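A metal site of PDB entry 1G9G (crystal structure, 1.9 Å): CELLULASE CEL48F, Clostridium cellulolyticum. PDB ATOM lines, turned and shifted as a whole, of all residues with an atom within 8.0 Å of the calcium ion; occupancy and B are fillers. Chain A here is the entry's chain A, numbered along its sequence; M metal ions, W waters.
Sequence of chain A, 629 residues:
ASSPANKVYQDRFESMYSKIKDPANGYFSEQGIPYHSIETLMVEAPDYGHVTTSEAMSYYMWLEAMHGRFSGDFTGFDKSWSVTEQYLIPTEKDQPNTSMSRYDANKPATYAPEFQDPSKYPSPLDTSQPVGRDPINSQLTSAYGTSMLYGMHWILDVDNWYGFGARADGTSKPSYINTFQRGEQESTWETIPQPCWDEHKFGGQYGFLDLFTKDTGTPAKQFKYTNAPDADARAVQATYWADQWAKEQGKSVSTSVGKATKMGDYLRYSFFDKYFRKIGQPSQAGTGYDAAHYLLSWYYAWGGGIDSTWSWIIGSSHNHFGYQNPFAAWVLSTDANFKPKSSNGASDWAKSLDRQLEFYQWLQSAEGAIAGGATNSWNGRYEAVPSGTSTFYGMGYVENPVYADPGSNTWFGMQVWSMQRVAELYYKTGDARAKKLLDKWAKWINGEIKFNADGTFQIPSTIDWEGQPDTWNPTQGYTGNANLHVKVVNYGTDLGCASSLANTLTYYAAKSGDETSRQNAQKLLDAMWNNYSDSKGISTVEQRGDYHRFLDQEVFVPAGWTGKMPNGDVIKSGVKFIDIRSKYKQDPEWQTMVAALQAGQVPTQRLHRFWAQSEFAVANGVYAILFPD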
ATOM      1  N   GLN A 116      21.096   6.434  29.527  1.00  0.00           N
ATOM      2  CA  GLN A 116      19.707   6.392  29.078  1.00  0.00           C
ATOM      3  C   GLN A 116      19.414   5.382  27.967  1.00  0.00           C
ATOM      4  O   GLN A 116      18.294   5.332  27.443  1.00  0.00           O
ATOM      5  CB  GLN A 116      19.252   7.793  28.639  1.00  0.00           C
ATOM      6  CG  GLN A 116      18.954   8.732  29.809  1.00  0.00           C
ATOM      7  CD  GLN A 116      20.162   8.948  30.709  1.00  0.00           C
ATOM      8  OE1 GLN A 116      21.188   9.473  30.282  1.00  0.00           O
ATOM      9  NE2 GLN A 116      20.038   8.548  31.977  1.00  0.00           N
ATOM     10  N   ASP A 117      20.416   4.597  27.586  1.00  0.00           N
ATOM     11  CA  ASP A 117      20.223   3.571  26.583  1.00  0.00           C
ATOM     12  C   ASP A 117      21.101   2.380  26.919  1.00  0.00           C
ATOM     13  O   ASP A 117      22.289   2.552  27.198  1.00  0.00           O
ATOM     14  CB  ASP A 117      20.584   4.078  25.184  1.00  0.00           C
ATOM     15  CG  ASP A 117      20.085   3.150  24.091  1.00  0.00           C
ATOM     16  OD1 ASP A 117      18.886   3.248  23.739  1.00  0.00           O
ATOM     17  OD2 ASP A 117      20.860   2.310  23.597  1.00  0.00           O
ATOM     18  N   PRO A 118      20.541   1.169  26.890  1.00  0.00           N
ATOM     19  CA  PRO A 118      21.299  -0.036  27.206  1.00  0.00           C
ATOM     20  C   PRO A 118      22.541  -0.249  26.351  1.00  0.00           C
ATOM     21  O   PRO A 118      23.480  -0.921  26.776  1.00  0.00           O
ATOM     22  CB  PRO A 118      20.268  -1.158  26.992  1.00  0.00           C
ATOM     23  CG  PRO A 118      18.973  -0.478  27.313  1.00  0.00           C
ATOM     24  CD  PRO A 118      19.125   0.850  26.616  1.00  0.00           C
ATOM     25  N   GLY A 183      19.979   0.773  33.122  1.00  0.00           N
ATOM     26  CA  GLY A 183      19.238   2.023  32.976  1.00  0.00           C
ATOM     27  C   GLY A 183      17.746   2.059  32.733  1.00  0.00           C
ATOM     28  O   GLY A 183      17.083   1.025  32.591  1.00  0.00           O
ATOM     29  N   GLU A 184      17.231   3.290  32.656  1.00  0.00           N
ATOM     30  CA  GLU A 184      15.815   3.569  32.474  1.00  0.00           C
ATOM     31  C   GLU A 184      15.154   3.013  31.218  1.00  0.00           C
ATOM     32  O   GLU A 184      13.932   2.844  31.186  1.00  0.00           O
ATOM     33  CB  GLU A 184      15.572   5.088  32.517  1.00  0.00           C
ATOM     34  CG  GLU A 184      16.268   5.876  31.415  1.00  0.00           C
ATOM     35  CD  GLU A 184      15.796   7.314  31.321  1.00  0.00           C
ATOM     36  OE1 GLU A 184      15.633   7.958  32.373  1.00  0.00           O
ATOM     37  OE2 GLU A 184      15.580   7.804  30.188  1.00  0.00           O
ATOM     38  N   GLN A 185      15.939   2.737  30.185  1.00  0.00           N
ATOM     39  CA  GLN A 185      15.350   2.210  28.961  1.00  0.00           C
ATOM     40  C   GLN A 185      15.427   0.692  28.845  1.00  0.00           C
ATOM     41  O   GLN A 185      14.979   0.125  27.851  1.00  0.00           O
ATOM     42  CB  GLN A 185      15.999   2.853  27.725  1.00  0.00           C
ATOM     43  CG  GLN A 185      15.176   3.994  27.139  1.00  0.00           C
ATOM     44  CD  GLN A 185      13.746   3.566  26.795  1.00  0.00           C
ATOM     45  OE1 GLN A 185      13.521   2.475  26.267  1.00  0.00           O
ATOM     46  NE2 GLN A 185      12.779   4.431  27.095  1.00  0.00           N
ATOM     47  N   GLU A 186      15.984   0.039  29.850  1.00  0.00           N
ATOM     48  CA  GLU A 186      16.070  -1.411  29.799  1.00  0.00           C
ATOM     49  C   GLU A 186      14.785  -1.998  30.388  1.00  0.00           C
ATOM     50  O   GLU A 186      14.654  -2.113  31.599  1.00  0.00           O
ATOM     51  CB  GLU A 186      17.271  -1.935  30.585  1.00  0.00           C
ATOM     52  CG  GLU A 186      17.441  -3.443  30.458  1.00  0.00           C
ATOM     53  CD  GLU A 186      18.601  -3.999  31.259  1.00  0.00           C
ATOM     54  OE1 GLU A 186      18.687  -3.700  32.469  1.00  0.00           O
ATOM     55  OE2 GLU A 186      19.434  -4.742  30.688  1.00  0.00           O
ATOM     56  N   SER A 187      13.850  -2.360  29.520  1.00  0.00           N
ATOM     57  CA  SER A 187      12.590  -2.951  29.983  1.00  0.00           C
ATOM     58  C   SER A 187      12.860  -4.401  30.371  1.00  0.00           C
ATOM     59  O   SER A 187      13.962  -4.905  30.193  1.00  0.00           O
ATOM     60  CB  SER A 187      11.559  -2.938  28.873  1.00  0.00           C
ATOM     61  OG  SER A 187      11.923  -3.858  27.855  1.00  0.00           O
ATOM     62  N   THR A 188      11.822  -5.051  30.884  1.00  0.00           N
ATOM     63  CA  THR A 188      11.897  -6.449  31.294  1.00  0.00           C
ATOM     64  C   THR A 188      12.288  -7.316  30.098  1.00  0.00           C
ATOM     65  O   THR A 188      12.884  -8.377  30.264  1.00  0.00           O
ATOM     66  CB  THR A 188      10.540  -6.927  31.831  1.00  0.00           C
ATOM     67  OG1 THR A 188      10.121  -6.063  32.896  1.00  0.00           O
ATOM     68  CG2 THR A 188      10.646  -8.355  32.349  1.00  0.00           C
ATOM     69  N   TRP A 189      11.952  -6.853  28.901  1.00  0.00           N
ATOM     70  CA  TRP A 189      12.244  -7.593  27.673  1.00  0.00           C
ATOM     71  C   TRP A 189      13.667  -7.418  27.139  1.00  0.00           C
ATOM     72  O   TRP A 189      14.084  -8.150  26.245  1.00  0.00           O
ATOM     73  CB  TRP A 189      11.274  -7.172  26.562  1.00  0.00           C
ATOM     74  CG  TRP A 189       9.826  -7.200  26.959  1.00  0.00           C
ATOM     75  CD1 TRP A 189       9.101  -6.187  27.496  1.00  0.00           C
ATOM     76  CD2 TRP A 189       8.941  -8.328  26.857  1.00  0.00           C
ATOM     77  NE1 TRP A 189       7.811  -6.603  27.739  1.00  0.00           N
ATOM     78  CE2 TRP A 189       7.687  -7.911  27.355  1.00  0.00           C
ATOM     79  CE3 TRP A 189       9.092  -9.639  26.392  1.00  0.00           C
ATOM     80  CZ2 TRP A 189       6.583  -8.771  27.411  1.00  0.00           C
ATOM     81  CZ3 TRP A 189       7.994 -10.494  26.442  1.00  0.00           C
ATOM     82  CH2 TRP A 189       6.757 -10.052  26.944  1.00  0.00           C
ATOM     83  N   GLU A 190      14.419  -6.468  27.702  1.00  0.00           N
ATOM     84  CA  GLU A 190      15.765  -6.176  27.216  1.00  0.00           C
ATOM     85  C   GLU A 190      16.908  -6.536  28.142  1.00  0.00           C
ATOM     86  O   GLU A 190      18.049  -6.094  27.932  1.00  0.00           O
ATOM     87  CB  GLU A 190      15.856  -4.693  26.865  1.00  0.00           C
ATOM     88  CG  GLU A 190      14.812  -4.267  25.848  1.00  0.00           C
ATOM     89  CD  GLU A 190      14.631  -2.761  25.796  1.00  0.00           C
ATOM     90  OE1 GLU A 190      15.443  -2.077  25.144  1.00  0.00           O
ATOM     91  OE2 GLU A 190      13.671  -2.278  26.420  1.00  0.00           O
ATOM     92  N   ALA A 404      11.538   4.047  32.251  1.00  0.00           N
ATOM     93  CA  ALA A 404      10.729   4.749  31.256  1.00  0.00           C
ATOM     94  C   ALA A 404      10.132   3.821  30.210  1.00  0.00           C
ATOM     95  O   ALA A 404       9.407   4.281  29.319  1.00  0.00           O
ATOM     96  CB  ALA A 404      11.594   5.812  30.570  1.00  0.00           C
ATOM     97  N   ASP A 405      10.385   2.517  30.319  1.00  0.00           N
ATOM     98  CA  ASP A 405       9.881   1.556  29.343  1.00  0.00           C
ATOM     99  C   ASP A 405       9.194   0.363  30.025  1.00  0.00           C
ATOM    100  O   ASP A 405       9.782  -0.714  30.153  1.00  0.00           O
ATOM    101  CB  ASP A 405      11.067   1.076  28.476  1.00  0.00           C
ATOM    102  CG  ASP A 405      10.644   0.196  27.302  1.00  0.00           C
ATOM    103  OD1 ASP A 405       9.431   0.041  27.043  1.00  0.00           O
ATOM    104  OD2 ASP A 405      11.545  -0.343  26.637  1.00  0.00           O
ATOM    105  N   PRO A 406       7.935   0.539  30.468  1.00  0.00           N
ATOM    106  CA  PRO A 406       7.113   1.751  30.389  1.00  0.00           C
ATOM    107  C   PRO A 406       7.370   2.682  31.581  1.00  0.00           C
ATOM    108  O   PRO A 406       8.066   2.298  32.520  1.00  0.00           O
ATOM    109  CB  PRO A 406       5.693   1.195  30.383  1.00  0.00           C
ATOM    110  CG  PRO A 406       5.814   0.063  31.340  1.00  0.00           C
ATOM    111  CD  PRO A 406       7.121  -0.604  30.943  1.00  0.00           C
ATOM    112  N   ARG A 549       6.745  -8.492  22.043  1.00  0.00           N
ATOM    113  CA  ARG A 549       8.171  -8.304  22.318  1.00  0.00           C
ATOM    114  C   ARG A 549       8.874  -9.636  22.573  1.00  0.00           C
ATOM    115  O   ARG A 549      10.095  -9.728  22.507  1.00  0.00           O
ATOM    116  CB  ARG A 549       8.347  -7.346  23.498  1.00  0.00           C
ATOM    117  CG  ARG A 549       7.711  -5.987  23.202  1.00  0.00           C
ATOM    118  CD  ARG A 549       7.916  -4.968  24.314  1.00  0.00           C
ATOM    119  NE  ARG A 549       9.249  -4.376  24.308  1.00  0.00           N
ATOM    120  CZ  ARG A 549       9.591  -3.303  25.009  1.00  0.00           C
ATOM    121  NH1 ARG A 549       8.700  -2.723  25.800  1.00  0.00           N
ATOM    122  NH2 ARG A 549      10.817  -2.814  24.925  1.00  0.00           N
ATOM    123  N   GLN A 553      11.696  -8.267  20.161  1.00  0.00           N
ATOM    124  CA  GLN A 553      12.544  -7.378  20.954  1.00  0.00           C
ATOM    125  C   GLN A 553      13.999  -7.833  20.900  1.00  0.00           C
ATOM    126  O   GLN A 553      14.337  -8.898  21.392  1.00  0.00           O
ATOM    127  CB  GLN A 553      12.090  -7.332  22.409  1.00  0.00           C
ATOM    128  CG  GLN A 553      12.957  -6.432  23.298  1.00  0.00           C
ATOM    129  CD  GLN A 553      12.898  -4.972  22.888  1.00  0.00           C
ATOM    130  OE1 GLN A 553      11.838  -4.346  22.962  1.00  0.00           O
ATOM    131  NE2 GLN A 553      14.027  -4.420  22.474  1.00  0.00           N
ATOM    132  N   GLU A 554      14.855  -7.017  20.302  1.00  0.00           N
ATOM    133  CA  GLU A 554      16.269  -7.351  20.221  1.00  0.00           C
ATOM    134  C   GLU A 554      16.904  -7.019  21.565  1.00  0.00           C
ATOM    135  O   GLU A 554      16.551  -6.041  22.213  1.00  0.00           O
ATOM    136  CB  GLU A 554      16.953  -6.536  19.128  1.00  0.00           C
ATOM    137  CG  GLU A 554      18.401  -6.927  18.888  1.00  0.00           C
ATOM    138  CD  GLU A 554      19.080  -6.079  17.833  1.00  0.00           C
ATOM    139  OE1 GLU A 554      18.511  -5.931  16.717  1.00  0.00           O
ATOM    140  OE2 GLU A 554      20.179  -5.547  18.099  1.00  0.00           O
HETATM  141 CA    CA M   1      13.826  -0.024  25.821  1.00  0.00          CA
HETATM  142  O   HOH W   1      12.768  -0.185  23.662  1.00  0.00           O
HETATM  143  O   HOH W   2      15.666   0.991  24.600  1.00  0.00           O
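The calcium ion is bound by OE2 of Glu 190, O of Gln 185, water W1, water W2, OD2 of Asp 405, OE1 of Gln 185 and OE1 of Glu 190.
The calcium ion has seven donor atoms within binding distance.
OE2 of Glu 190 lies close to OG of Ser 187 (2.8 Å).
NH1 of Arg 549 lies within salt-bridge range of OD1 of Asp 405 (3.1 Å).
The guanidinium group (NH2) of Arg 549 sits close to the side-chain carboxylate (OE2) of Glu 190 (3.3 Å).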
